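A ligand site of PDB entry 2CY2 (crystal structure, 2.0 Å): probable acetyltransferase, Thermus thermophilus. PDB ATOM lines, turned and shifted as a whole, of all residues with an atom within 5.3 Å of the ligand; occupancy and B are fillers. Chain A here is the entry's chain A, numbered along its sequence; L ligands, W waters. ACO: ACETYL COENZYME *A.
N of Gly 136 lies within hydrogen-bond range of OD1 of Asn 133 (3.1 Å). OH of Tyr 95 sits at hydrogen-bond distance from OH of Tyr 26, at 2.8 Å. O of Gln 101 lies within hydrogen-bond range of NZ of Lys 103 (3.4 Å). The side-chain amide oxygen of Asn 133 sits close to the backbone NH of Lys 135 (3.3 Å). NZ of Lys 135 is in hydrogen-bond range of OE1 of Gln 101, at 2.6 Å. The backbone carbonyl oxygen (O) of Val 96 lies within hydrogen-bond range of the side-chain amide nitrogen (NE2) of Gln 101 (2.9 Å). The side-chain hydroxyl of Thr 25 sits at hydrogen-bond distance from the backbone carbonyl oxygen of Thr 21.
The backbone carbonyl oxygen (O) of Trp 128 sits close to a sulfur (S1P) of the ligand (3.6 Å). Residues that only touch the ligand: Thr 21 (3.8 Å), Thr 25 (3.1 Å), Tyr 26 (3.7 Å), Ala 93 (3.5 Å), Leu 105 (3.6 Å), Val 127 (3.9 Å), Val 129 (3.98 Å), Pro 134 (3.6 Å), Gly 136 (3.6 Å), Gly 138 (3.4 Å), Phe 139 (3.4 Å) and Leu 143 (3.9997 Å). Hydrophobic or aromatic side chains within 4 Å of the ligand: Ile 94, Tyr 95, Val 127, Val 129, Phe 139, Tyr 140, His 142 and Leu 143. Within 4 Å of the ligand: Thr 21, Thr 25, Tyr 26, Ala 93, Ile 94, Tyr 95, Val 96, Gln 101, Arg 102, Lys 103, Gly 104, Leu 105, Gly 106, Arg 107, Val 127, Trp 128, Val 129, Asn 133, Pro 134, Lys 135, Gly 136, Gly 138, Phe 139, Tyr 140, His 142 and Leu 143. The nearest printed residue that does not touch the ligand is Leu 91 (4.2 Å).
Water W5 bridges N7A of the ligand (2.8 Å) and O of Lys 135 (3.2 Å). Water W2 bridges the guanidinium group of Arg 102 (3.0 Å) and an oxygen (O2B) of the ligand (3.0 Å). Water W7 lies within hydrogen-bond range of the backbone carbonyl oxygen (O) of Trp 128 (2.8 Å) and the backbone carbonyl oxygen (O) of Trp 92 (3.2 Å). Water W8 lies within hydrogen-bond range of O of the ligand (3.4 Å), O of Trp 92 (3.4 Å) and OH of Tyr 95 (3.5 Å).
The backbone NH (N) of Gly 104 sits at hydrogen-bond distance from an oxygen (O1A) of the ligand, at 2.8 Å. The backbone carbonyl oxygen (O) of Lys 135 is in hydrogen-bond range of a nitrogen (N6A) of the ligand (3.0 Å). N4P of the ligand is in hydrogen-bond range of O of Ile 94 (2.9 Å). N of Lys 103 lies within hydrogen-bond range of O1A of the ligand (3.2 Å). A ring nitrogen (NE2) of His 142 lies within hydrogen-bond range of an oxygen (O8A) of the ligand (2.7 Å). An oxygen (O5P) of the ligand lies within hydrogen-bond range of the side-chain amide nitrogen of Asn 133, 2.7 Å away. NE2 of Gln 101 lies close to N8P of the ligand. O of the ligand lies within hydrogen-bond range of OH of Tyr 95. An oxygen (O2A) of the ligand is in hydrogen-bond range of the backbone NH (N) of Arg 107. A sulfur (S1P) of the ligand sits close to the side-chain hydroxyl of Tyr 140. The guanidinium group (NH1) of Arg 107 is in salt-bridge range of an oxygen (O9A) of the ligand (3.4 Å). An oxygen (O2B) of the ligand lies within hydrogen-bond range of the guanidinium group (NH2) of Arg 102 (3.0 Å). An oxygen (O4A) of the ligand is in hydrogen-bond range of the backbone NH (N) of Arg 102 (3.0 Å). N of Gly 106 lies within hydrogen-bond range of O5A of the ligand, 2.8 Å away. The backbone NH (N) of Val 96 lies within hydrogen-bond range of an oxygen (O9P) of the ligand, 2.9 Å away.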
ATOM      1  N   THR A  21      10.209 -21.723  18.631  1.00  0.00           N
ATOM      2  CA  THR A  21      11.437 -20.928  18.726  1.00  0.00           C
ATOM      3  C   THR A  21      12.377 -21.244  17.552  1.00  0.00           C
ATOM      4  O   THR A  21      13.069 -20.352  17.046  1.00  0.00           O
ATOM      5  CB  THR A  21      12.146 -21.127  20.068  1.00  0.00           C
ATOM      6  OG1 THR A  21      11.182 -20.991  21.129  1.00  0.00           O
ATOM      7  CG2 THR A  21      13.202 -20.041  20.262  1.00  0.00           C
ATOM      8  N   THR A  25      13.666 -18.352  15.316  1.00  0.00           N
ATOM      9  CA  THR A  25      15.089 -18.062  15.296  1.00  0.00           C
ATOM     10  C   THR A  25      15.819 -18.355  13.996  1.00  0.00           C
ATOM     11  O   THR A  25      16.706 -17.602  13.614  1.00  0.00           O
ATOM     12  CB  THR A  25      15.853 -18.831  16.420  1.00  0.00           C
ATOM     13  OG1 THR A  25      15.192 -18.624  17.665  1.00  0.00           O
ATOM     14  CG2 THR A  25      17.319 -18.354  16.525  1.00  0.00           C
ATOM     15  N   TYR A  26      15.449 -19.443  13.320  1.00  0.00           N
ATOM     16  CA  TYR A  26      16.188 -19.822  12.131  1.00  0.00           C
ATOM     17  C   TYR A  26      15.639 -19.391  10.780  1.00  0.00           C
ATOM     18  O   TYR A  26      16.085 -19.891   9.744  1.00  0.00           O
ATOM     19  CB  TYR A  26      16.477 -21.324  12.158  1.00  0.00           C
ATOM     20  CG  TYR A  26      17.178 -21.771  13.430  1.00  0.00           C
ATOM     21  CD1 TYR A  26      18.297 -21.079  13.898  1.00  0.00           C
ATOM     22  CD2 TYR A  26      16.693 -22.839  14.178  1.00  0.00           C
ATOM     23  CE1 TYR A  26      18.921 -21.437  15.109  1.00  0.00           C
ATOM     24  CE2 TYR A  26      17.300 -23.221  15.388  1.00  0.00           C
ATOM     25  CZ  TYR A  26      18.414 -22.506  15.858  1.00  0.00           C
ATOM     26  OH  TYR A  26      18.998 -22.851  17.073  1.00  0.00           O
ATOM     27  N   LEU A  91      25.409 -29.212  26.160  1.00  0.00           N
ATOM     28  CA  LEU A  91      24.094 -28.596  26.350  1.00  0.00           C
ATOM     29  C   LEU A  91      23.416 -28.998  25.020  1.00  0.00           C
ATOM     30  O   LEU A  91      23.721 -28.450  23.956  1.00  0.00           O
ATOM     31  CB  LEU A  91      24.227 -27.063  26.446  1.00  0.00           C
ATOM     32  CG  LEU A  91      23.137 -26.299  27.224  1.00  0.00           C
ATOM     33  CD1 LEU A  91      23.345 -24.786  27.079  1.00  0.00           C
ATOM     34  CD2 LEU A  91      21.767 -26.695  26.728  1.00  0.00           C
ATOM     35  N   TRP A  92      22.537 -29.986  25.067  1.00  0.00           N
ATOM     36  CA  TRP A  92      21.900 -30.458  23.833  1.00  0.00           C
ATOM     37  C   TRP A  92      20.952 -29.454  23.199  1.00  0.00           C
ATOM     38  O   TRP A  92      20.915 -29.300  21.971  1.00  0.00           O
ATOM     39  CB  TRP A  92      21.142 -31.773  24.106  1.00  0.00           C
ATOM     40  CG  TRP A  92      22.063 -32.897  24.449  1.00  0.00           C
ATOM     41  CD1 TRP A  92      23.417 -32.932  24.310  1.00  0.00           C
ATOM     42  CD2 TRP A  92      21.686 -34.171  24.969  1.00  0.00           C
ATOM     43  NE1 TRP A  92      23.913 -34.140  24.719  1.00  0.00           N
ATOM     44  CE2 TRP A  92      22.875 -34.927  25.132  1.00  0.00           C
ATOM     45  CE3 TRP A  92      20.467 -34.754  25.329  1.00  0.00           C
ATOM     46  CZ2 TRP A  92      22.874 -36.232  25.630  1.00  0.00           C
ATOM     47  CZ3 TRP A  92      20.466 -36.059  25.827  1.00  0.00           C
ATOM     48  CH2 TRP A  92      21.667 -36.777  25.974  1.00  0.00           C
ATOM     49  N   ALA A  93      20.222 -28.728  24.047  1.00  0.00           N
ATOM     50  CA  ALA A  93      19.256 -27.758  23.535  1.00  0.00           C
ATOM     51  C   ALA A  93      18.820 -26.786  24.612  1.00  0.00           C
ATOM     52  O   ALA A  93      18.736 -27.144  25.772  1.00  0.00           O
ATOM     53  CB  ALA A  93      18.017 -28.493  23.020  1.00  0.00           C
ATOM     54  N   ILE A  94      18.570 -25.562  24.192  1.00  0.00           N
ATOM     55  CA  ILE A  94      18.039 -24.564  25.100  1.00  0.00           C
ATOM     56  C   ILE A  94      17.293 -23.573  24.224  1.00  0.00           C
ATOM     57  O   ILE A  94      17.813 -23.018  23.237  1.00  0.00           O
ATOM     58  CB  ILE A  94      19.151 -23.894  25.977  1.00  0.00           C
ATOM     59  CG1 ILE A  94      18.478 -22.901  26.945  1.00  0.00           C
ATOM     60  CG2 ILE A  94      20.194 -23.232  25.100  1.00  0.00           C
ATOM     61  CD1 ILE A  94      19.424 -22.270  27.969  1.00  0.00           C
ATOM     62  N   TYR A  95      16.011 -23.384  24.569  1.00  0.00           N
ATOM     63  CA  TYR A  95      15.119 -22.488  23.862  1.00  0.00           C
ATOM     64  C   TYR A  95      14.142 -21.818  24.810  1.00  0.00           C
ATOM     65  O   TYR A  95      13.591 -22.471  25.729  1.00  0.00           O
ATOM     66  CB  TYR A  95      14.323 -23.255  22.791  1.00  0.00           C
ATOM     67  CG  TYR A  95      15.197 -23.776  21.645  1.00  0.00           C
ATOM     68  CD1 TYR A  95      15.821 -25.030  21.720  1.00  0.00           C
ATOM     69  CD2 TYR A  95      15.493 -22.955  20.556  1.00  0.00           C
ATOM     70  CE1 TYR A  95      16.744 -25.451  20.707  1.00  0.00           C
ATOM     71  CE2 TYR A  95      16.399 -23.352  19.566  1.00  0.00           C
ATOM     72  CZ  TYR A  95      17.026 -24.584  19.638  1.00  0.00           C
ATOM     73  OH  TYR A  95      17.956 -24.893  18.660  1.00  0.00           O
ATOM     74  N   VAL A  96      13.935 -20.522  24.596  1.00  0.00           N
ATOM     75  CA  VAL A  96      12.965 -19.746  25.387  1.00  0.00           C
ATOM     76  C   VAL A  96      12.078 -19.022  24.335  1.00  0.00           C
ATOM     77  O   VAL A  96      12.594 -18.441  23.374  1.00  0.00           O
ATOM     78  CB  VAL A  96      13.666 -18.662  26.273  1.00  0.00           C
ATOM     79  CG1 VAL A  96      12.593 -17.785  26.987  1.00  0.00           C
ATOM     80  CG2 VAL A  96      14.627 -19.354  27.276  1.00  0.00           C
ATOM     81  N   TRP A 100       9.520 -14.266  25.729  1.00  0.00           N
ATOM     82  CA  TRP A 100       9.932 -14.428  27.118  1.00  0.00           C
ATOM     83  C   TRP A 100      11.463 -14.345  27.234  1.00  0.00           C
ATOM     84  O   TRP A 100      12.009 -14.526  28.336  1.00  0.00           O
ATOM     85  CB  TRP A 100       9.451 -15.772  27.663  1.00  0.00           C
ATOM     86  CG  TRP A 100       8.165 -15.693  28.465  1.00  0.00           C
ATOM     87  CD1 TRP A 100       8.035 -15.383  29.792  1.00  0.00           C
ATOM     88  CD2 TRP A 100       6.851 -15.991  27.996  1.00  0.00           C
ATOM     89  NE1 TRP A 100       6.713 -15.480  30.185  1.00  0.00           N
ATOM     90  CE2 TRP A 100       5.964 -15.850  29.100  1.00  0.00           C
ATOM     91  CE3 TRP A 100       6.336 -16.368  26.738  1.00  0.00           C
ATOM     92  CZ2 TRP A 100       4.586 -16.082  28.995  1.00  0.00           C
ATOM     93  CZ3 TRP A 100       4.952 -16.596  26.620  1.00  0.00           C
ATOM     94  CH2 TRP A 100       4.097 -16.454  27.744  1.00  0.00           C
ATOM     95  N   GLN A 101      12.137 -14.089  26.113  1.00  0.00           N
ATOM     96  CA  GLN A 101      13.600 -13.965  26.063  1.00  0.00           C
ATOM     97  C   GLN A 101      14.077 -12.679  26.754  1.00  0.00           C
ATOM     98  O   GLN A 101      13.276 -11.745  26.960  1.00  0.00           O
ATOM     99  CB  GLN A 101      14.094 -13.968  24.601  1.00  0.00           C
ATOM    100  CG  GLN A 101      14.088 -15.376  23.964  1.00  0.00           C
ATOM    101  CD  GLN A 101      14.298 -15.348  22.456  1.00  0.00           C
ATOM    102  OE1 GLN A 101      14.735 -14.354  21.884  1.00  0.00           O
ATOM    103  NE2 GLN A 101      13.969 -16.455  21.806  1.00  0.00           N
ATOM    104  N   ARG A 102      15.363 -12.641  27.093  1.00  0.00           N
ATOM    105  CA  ARG A 102      16.018 -11.503  27.754  1.00  0.00           C
ATOM    106  C   ARG A 102      15.338 -11.083  29.053  1.00  0.00           C
ATOM    107  O   ARG A 102      15.249  -9.896  29.367  1.00  0.00           O
ATOM    108  CB  ARG A 102      16.136 -10.291  26.799  1.00  0.00           C
ATOM    109  CG  ARG A 102      16.861 -10.590  25.467  1.00  0.00           C
ATOM    110  CD  ARG A 102      18.236 -11.295  25.645  1.00  0.00           C
ATOM    111  NE  ARG A 102      19.304 -10.387  26.094  1.00  0.00           N
ATOM    112  CZ  ARG A 102      20.037  -9.604  25.290  1.00  0.00           C
ATOM    113  NH1 ARG A 102      19.846  -9.619  23.979  1.00  0.00           N
ATOM    114  NH2 ARG A 102      20.966  -8.802  25.805  1.00  0.00           N
ATOM    115  N   LYS A 103      14.860 -12.070  29.801  1.00  0.00           N
ATOM    116  CA  LYS A 103      14.236 -11.864  31.103  1.00  0.00           C
ATOM    117  C   LYS A 103      14.930 -12.786  32.124  1.00  0.00           C
ATOM    118  O   LYS A 103      14.404 -13.057  33.207  1.00  0.00           O
ATOM    119  CB  LYS A 103      12.751 -12.230  31.074  1.00  0.00           C
ATOM    120  CG  LYS A 103      11.896 -11.340  30.231  1.00  0.00           C
ATOM    121  CD  LYS A 103      10.466 -11.860  30.249  1.00  0.00           C
ATOM    122  CE  LYS A 103       9.584 -10.995  29.385  1.00  0.00           C
ATOM    123  NZ  LYS A 103      10.156 -10.849  27.997  1.00  0.00           N
ATOM    124  N   GLY A 104      16.108 -13.303  31.735  1.00  0.00           N
ATOM    125  CA  GLY A 104      16.856 -14.169  32.627  1.00  0.00           C
ATOM    126  C   GLY A 104      16.473 -15.638  32.641  1.00  0.00           C
ATOM    127  O   GLY A 104      17.076 -16.416  33.396  1.00  0.00           O
ATOM    128  N   LEU A 105      15.490 -16.060  31.828  1.00  0.00           N
ATOM    129  CA  LEU A 105      15.110 -17.487  31.853  1.00  0.00           C
ATOM    130  C   LEU A 105      16.198 -18.422  31.322  1.00  0.00           C
ATOM    131  O   LEU A 105      16.453 -19.468  31.933  1.00  0.00           O
ATOM    132  CB  LEU A 105      13.810 -17.720  31.090  1.00  0.00           C
ATOM    133  CG  LEU A 105      12.521 -17.392  31.865  1.00  0.00           C
ATOM    134  CD1 LEU A 105      12.606 -15.990  32.406  1.00  0.00           C
ATOM    135  CD2 LEU A 105      11.314 -17.548  30.949  1.00  0.00           C
ATOM    136  N   GLY A 106      16.838 -18.054  30.219  1.00  0.00           N
ATOM    137  CA  GLY A 106      17.886 -18.888  29.625  1.00  0.00           C
ATOM    138  C   GLY A 106      19.050 -19.057  30.602  1.00  0.00           C
ATOM    139  O   GLY A 106      19.595 -20.156  30.774  1.00  0.00           O
ATOM    140  N   ARG A 107      19.428 -17.964  31.244  1.00  0.00           N
ATOM    141  CA  ARG A 107      20.522 -18.017  32.207  1.00  0.00           C
ATOM    142  C   ARG A 107      20.164 -18.972  33.348  1.00  0.00           C
ATOM    143  O   ARG A 107      20.984 -19.794  33.766  1.00  0.00           O
ATOM    144  CB  ARG A 107      20.813 -16.619  32.785  1.00  0.00           C
ATOM    145  CG  ARG A 107      22.107 -16.582  33.628  1.00  0.00           C
ATOM    146  CD  ARG A 107      21.996 -15.531  34.740  1.00  0.00           C
ATOM    147  NE  ARG A 107      23.137 -15.537  35.660  1.00  0.00           N
ATOM    148  CZ  ARG A 107      24.347 -15.070  35.361  1.00  0.00           C
ATOM    149  NH1 ARG A 107      24.591 -14.557  34.158  1.00  0.00           N
ATOM    150  NH2 ARG A 107      25.314 -15.105  36.284  1.00  0.00           N
ATOM    151  N   ALA A 108      18.933 -18.869  33.843  1.00  0.00           N
ATOM    152  CA  ALA A 108      18.477 -19.725  34.944  1.00  0.00           C
ATOM    153  C   ALA A 108      18.496 -21.216  34.524  1.00  0.00           C
ATOM    154  O   ALA A 108      18.902 -22.097  35.314  1.00  0.00           O
ATOM    155  CB  ALA A 108      17.052 -19.309  35.356  1.00  0.00           C
ATOM    156  N   VAL A 127      28.820 -26.583  23.832  1.00  0.00           N
ATOM    157  CA  VAL A 127      27.515 -26.379  23.191  1.00  0.00           C
ATOM    158  C   VAL A 127      27.740 -26.025  21.729  1.00  0.00           C
ATOM    159  O   VAL A 127      28.650 -25.251  21.386  1.00  0.00           O
ATOM    160  CB  VAL A 127      26.698 -25.244  23.875  1.00  0.00           C
ATOM    161  CG1 VAL A 127      27.427 -23.905  23.748  1.00  0.00           C
ATOM    162  CG2 VAL A 127      25.292 -25.139  23.208  1.00  0.00           C
ATOM    163  N   TRP A 128      26.925 -26.606  20.846  1.00  0.00           N
ATOM    164  CA  TRP A 128      27.018 -26.328  19.402  1.00  0.00           C
ATOM    165  C   TRP A 128      25.895 -25.362  19.037  1.00  0.00           C
ATOM    166  O   TRP A 128      24.742 -25.514  19.482  1.00  0.00           O
ATOM    167  CB  TRP A 128      26.883 -27.609  18.572  1.00  0.00           C
ATOM    168  CG  TRP A 128      28.108 -28.482  18.626  1.00  0.00           C
ATOM    169  CD1 TRP A 128      28.318 -29.572  19.407  1.00  0.00           C
ATOM    170  CD2 TRP A 128      29.298 -28.296  17.854  1.00  0.00           C
ATOM    171  NE1 TRP A 128      29.558 -30.108  19.162  1.00  0.00           N
ATOM    172  CE2 TRP A 128      30.186 -29.345  18.211  1.00  0.00           C
ATOM    173  CE3 TRP A 128      29.696 -27.358  16.882  1.00  0.00           C
ATOM    174  CZ2 TRP A 128      31.465 -29.497  17.625  1.00  0.00           C
ATOM    175  CZ3 TRP A 128      30.979 -27.497  16.298  1.00  0.00           C
ATOM    176  CH2 TRP A 128      31.842 -28.557  16.678  1.00  0.00           C
ATOM    177  N   VAL A 129      26.237 -24.355  18.253  1.00  0.00           N
ATOM    178  CA  VAL A 129      25.260 -23.348  17.869  1.00  0.00           C
ATOM    179  C   VAL A 129      25.555 -22.939  16.437  1.00  0.00           C
ATOM    180  O   VAL A 129      26.741 -22.954  16.020  1.00  0.00           O
ATOM    181  CB  VAL A 129      25.360 -22.123  18.845  1.00  0.00           C
ATOM    182  CG1 VAL A 129      26.800 -21.680  18.933  1.00  0.00           C
ATOM    183  CG2 VAL A 129      24.453 -20.966  18.396  1.00  0.00           C
ATOM    184  N   ASN A 133      23.668 -17.819  14.041  1.00  0.00           N
ATOM    185  CA  ASN A 133      22.641 -17.563  15.055  1.00  0.00           C
ATOM    186  C   ASN A 133      23.245 -16.634  16.143  1.00  0.00           C
ATOM    187  O   ASN A 133      23.761 -17.109  17.175  1.00  0.00           O
ATOM    188  CB  ASN A 133      22.152 -18.890  15.672  1.00  0.00           C
ATOM    189  CG  ASN A 133      21.288 -18.672  16.912  1.00  0.00           C
ATOM    190  OD1 ASN A 133      20.793 -17.573  17.141  1.00  0.00           O
ATOM    191  ND2 ASN A 133      21.108 -19.725  17.706  1.00  0.00           N
ATOM    192  N   PRO A 134      23.192 -15.299  15.905  1.00  0.00           N
ATOM    193  CA  PRO A 134      23.702 -14.231  16.798  1.00  0.00           C
ATOM    194  C   PRO A 134      23.104 -14.249  18.190  1.00  0.00           C
ATOM    195  O   PRO A 134      23.779 -13.897  19.147  1.00  0.00           O
ATOM    196  CB  PRO A 134      23.313 -12.934  16.091  1.00  0.00           C
ATOM    197  CG  PRO A 134      23.090 -13.333  14.673  1.00  0.00           C
ATOM    198  CD  PRO A 134      22.535 -14.724  14.715  1.00  0.00           C
ATOM    199  N   LYS A 135      21.823 -14.625  18.269  1.00  0.00           N
ATOM    200  CA  LYS A 135      21.108 -14.697  19.554  1.00  0.00           C
ATOM    201  C   LYS A 135      21.767 -15.704  20.490  1.00  0.00           C
ATOM    202  O   LYS A 135      22.151 -15.365  21.627  1.00  0.00           O
ATOM    203  CB  LYS A 135      19.640 -15.155  19.361  1.00  0.00           C
ATOM    204  CG  LYS A 135      18.646 -14.112  18.901  1.00  0.00           C
ATOM    205  CD  LYS A 135      17.216 -14.396  19.417  1.00  0.00           C
ATOM    206  CE  LYS A 135      16.325 -13.207  19.083  1.00  0.00           C
ATOM    207  NZ  LYS A 135      14.893 -13.412  19.436  1.00  0.00           N
ATOM    208  N   GLY A 136      21.862 -16.935  20.015  1.00  0.00           N
ATOM    209  CA  GLY A 136      22.470 -17.967  20.828  1.00  0.00           C
ATOM    210  C   GLY A 136      23.948 -17.675  21.073  1.00  0.00           C
ATOM    211  O   GLY A 136      24.454 -17.853  22.183  1.00  0.00           O
ATOM    212  N   GLY A 138      25.576 -14.765  21.076  1.00  0.00           N
ATOM    213  CA  GLY A 138      25.735 -13.635  21.982  1.00  0.00           C
ATOM    214  C   GLY A 138      25.489 -14.057  23.406  1.00  0.00           C
ATOM    215  O   GLY A 138      26.187 -13.613  24.321  1.00  0.00           O
ATOM    216  N   PHE A 139      24.507 -14.936  23.592  1.00  0.00           N
ATOM    217  CA  PHE A 139      24.159 -15.464  24.918  1.00  0.00           C
ATOM    218  C   PHE A 139      25.341 -16.268  25.504  1.00  0.00           C
ATOM    219  O   PHE A 139      25.747 -16.068  26.657  1.00  0.00           O
ATOM    220  CB  PHE A 139      22.907 -16.396  24.787  1.00  0.00           C
ATOM    221  CG  PHE A 139      22.574 -17.190  26.026  1.00  0.00           C
ATOM    222  CD1 PHE A 139      22.104 -16.551  27.189  1.00  0.00           C
ATOM    223  CD2 PHE A 139      22.667 -18.594  26.020  1.00  0.00           C
ATOM    224  CE1 PHE A 139      21.726 -17.300  28.311  1.00  0.00           C
ATOM    225  CE2 PHE A 139      22.294 -19.338  27.149  1.00  0.00           C
ATOM    226  CZ  PHE A 139      21.810 -18.684  28.298  1.00  0.00           C
ATOM    227  N   TYR A 140      25.899 -17.186  24.715  1.00  0.00           N
ATOM    228  CA  TYR A 140      27.004 -18.008  25.214  1.00  0.00           C
ATOM    229  C   TYR A 140      28.244 -17.181  25.466  1.00  0.00           C
ATOM    230  O   TYR A 140      28.877 -17.347  26.506  1.00  0.00           O
ATOM    231  CB  TYR A 140      27.331 -19.150  24.250  1.00  0.00           C
ATOM    232  CG  TYR A 140      26.177 -20.151  24.193  1.00  0.00           C
ATOM    233  CD1 TYR A 140      25.666 -20.739  25.363  1.00  0.00           C
ATOM    234  CD2 TYR A 140      25.575 -20.450  22.979  1.00  0.00           C
ATOM    235  CE1 TYR A 140      24.562 -21.620  25.311  1.00  0.00           C
ATOM    236  CE2 TYR A 140      24.484 -21.322  22.900  1.00  0.00           C
ATOM    237  CZ  TYR A 140      23.990 -21.897  24.053  1.00  0.00           C
ATOM    238  OH  TYR A 140      22.956 -22.789  23.913  1.00  0.00           O
ATOM    239  N   HIS A 142      28.463 -14.049  26.207  1.00  0.00           N
ATOM    240  CA  HIS A 142      28.223 -13.263  27.408  1.00  0.00           C
ATOM    241  C   HIS A 142      28.423 -14.091  28.652  1.00  0.00           C
ATOM    242  O   HIS A 142      28.907 -13.591  29.661  1.00  0.00           O
ATOM    243  CB  HIS A 142      26.798 -12.690  27.428  1.00  0.00           C
ATOM    244  CG  HIS A 142      26.546 -11.741  28.552  1.00  0.00           C
ATOM    245  ND1 HIS A 142      27.121 -10.484  28.617  1.00  0.00           N
ATOM    246  CD2 HIS A 142      25.793 -11.867  29.683  1.00  0.00           C
ATOM    247  CE1 HIS A 142      26.736  -9.877  29.736  1.00  0.00           C
ATOM    248  NE2 HIS A 142      25.929 -10.698  30.397  1.00  0.00           N
ATOM    249  N   LEU A 143      28.042 -15.357  28.597  1.00  0.00           N
ATOM    250  CA  LEU A 143      28.142 -16.212  29.760  1.00  0.00           C
ATOM    251  C   LEU A 143      29.547 -16.762  30.026  1.00  0.00           C
ATOM    252  O   LEU A 143      29.759 -17.458  31.015  1.00  0.00           O
ATOM    253  CB  LEU A 143      27.120 -17.364  29.649  1.00  0.00           C
ATOM    254  CG  LEU A 143      25.864 -17.318  30.532  1.00  0.00           C
ATOM    255  CD1 LEU A 143      25.243 -15.925  30.518  1.00  0.00           C
ATOM    256  CD2 LEU A 143      24.845 -18.371  30.088  1.00  0.00           C
HETATM  257  N1A ACO L   1      23.861 -11.012  23.074  1.00  0.00           N
HETATM  258  C2A ACO L   1      24.456 -10.476  24.138  1.00  0.00           C
HETATM  259  N3A ACO L   1      24.055 -10.786  25.366  1.00  0.00           N
HETATM  260  C4A ACO L   1      23.051 -11.645  25.567  1.00  0.00           C
HETATM  261  C5A ACO L   1      22.415 -12.218  24.483  1.00  0.00           C
HETATM  262  C6A ACO L   1      22.845 -11.876  23.206  1.00  0.00           C
HETATM  263  N6A ACO L   1      22.286 -12.438  22.135  1.00  0.00           N
HETATM  264  N7A ACO L   1      21.492 -13.060  24.951  1.00  0.00           N
HETATM  265  C8A ACO L   1      21.549 -13.020  26.276  1.00  0.00           C
HETATM  266  N9A ACO L   1      22.500 -12.161  26.666  1.00  0.00           N
HETATM  267  C1B ACO L   1      22.860 -11.870  28.066  1.00  0.00           C
HETATM  268  C2B ACO L   1      21.696 -11.133  28.721  1.00  0.00           C
HETATM  269  O2B ACO L   1      21.874  -9.730  28.464  1.00  0.00           O
HETATM  270  C3B ACO L   1      21.993 -11.426  30.191  1.00  0.00           C
HETATM  271  O3B ACO L   1      23.063 -10.590  30.655  1.00  0.00           O
HETATM  272  P3B ACO L   1      23.135 -10.228  32.223  1.00  0.00           P
HETATM  273  O7A ACO L   1      22.007  -9.382  32.661  1.00  0.00           O
HETATM  274  O8A ACO L   1      24.568  -9.503  32.382  1.00  0.00           O
HETATM  275  O9A ACO L   1      23.206 -11.614  33.039  1.00  0.00           O
HETATM  276  C4B ACO L   1      22.445 -12.887  30.137  1.00  0.00           C
HETATM  277  O4B ACO L   1      22.984 -13.094  28.821  1.00  0.00           O
HETATM  278  C5B ACO L   1      21.273 -13.854  30.344  1.00  0.00           C
HETATM  279  O5B ACO L   1      20.273 -13.657  29.345  1.00  0.00           O
HETATM  280  P1A ACO L   1      18.827 -14.357  29.413  1.00  0.00           P
HETATM  281  O1A ACO L   1      17.771 -13.331  29.534  1.00  0.00           O
HETATM  282  O2A ACO L   1      18.827 -15.473  30.386  1.00  0.00           O
HETATM  283  O3A ACO L   1      18.769 -14.956  27.913  1.00  0.00           O
HETATM  284  P2A ACO L   1      17.488 -15.723  27.324  1.00  0.00           P
HETATM  285  O4A ACO L   1      17.013 -14.970  26.129  1.00  0.00           O
HETATM  286  O5A ACO L   1      16.523 -15.980  28.423  1.00  0.00           O
HETATM  287  O6A ACO L   1      18.101 -17.117  26.809  1.00  0.00           O
HETATM  288  CBP ACO L   1      18.602 -18.010  24.567  1.00  0.00           C
HETATM  289  CCP ACO L   1      19.076 -17.167  25.756  1.00  0.00           C
HETATM  290  CDP ACO L   1      19.687 -18.023  23.491  1.00  0.00           C
HETATM  291  CEP ACO L   1      18.381 -19.455  25.017  1.00  0.00           C
HETATM  292  CAP ACO L   1      17.302 -17.400  24.035  1.00  0.00           C
HETATM  293  OAP ACO L   1      17.549 -16.041  23.633  1.00  0.00           O
HETATM  294  C9P ACO L   1      16.723 -18.174  22.853  1.00  0.00           C
HETATM  295  O9P ACO L   1      15.981 -19.143  23.043  1.00  0.00           O
HETATM  296  N8P ACO L   1      17.094 -17.718  21.661  1.00  0.00           N
HETATM  297  C7P ACO L   1      16.664 -18.296  20.368  1.00  0.00           C
HETATM  298  C6P ACO L   1      16.955 -19.797  20.276  1.00  0.00           C
HETATM  299  C5P ACO L   1      18.452 -20.101  20.381  1.00  0.00           C
HETATM  300  O5P ACO L   1      19.287 -19.472  19.725  1.00  0.00           O
HETATM  301  N4P ACO L   1      18.763 -21.079  21.231  1.00  0.00           N
HETATM  302  C3P ACO L   1      20.142 -21.540  21.473  1.00  0.00           C
HETATM  303  C2P ACO L   1      20.530 -22.538  20.375  1.00  0.00           C
HETATM  304  S1P ACO L   1      22.098 -23.419  20.714  1.00  0.00           S
HETATM  305  C   ACO L   1      21.427 -25.017  21.312  1.00  0.00           C
HETATM  306  O   ACO L   1      20.128 -25.252  20.770  1.00  0.00           O
HETATM  307  CH3 ACO L   1      21.411 -25.072  22.839  1.00  0.00           C
HETATM  308  O   HOH W   1      20.003  -8.364  30.870  1.00  0.00           O
HETATM  309  O   HOH W   2      18.883  -9.363  28.864  1.00  0.00           O
HETATM  310  O   HOH W   3      20.163 -12.495  33.309  1.00  0.00           O
HETATM  311  O   HOH W   4      18.688 -11.084  30.895  1.00  0.00           O
HETATM  312  O   HOH W   5      19.610 -13.947  23.016  1.00  0.00           O
HETATM  313  O   HOH W   6      14.520 -14.841  29.504  1.00  0.00           O
HETATM  314  O   HOH W   7      22.966 -27.487  20.393  1.00  0.00           O
HETATM  315  O   HOH W   8      19.115 -28.122  19.352  1.00  0.00           O
HETATM  316  O   HOH W   9      27.401 -11.243  23.950  1.00  0.00           O
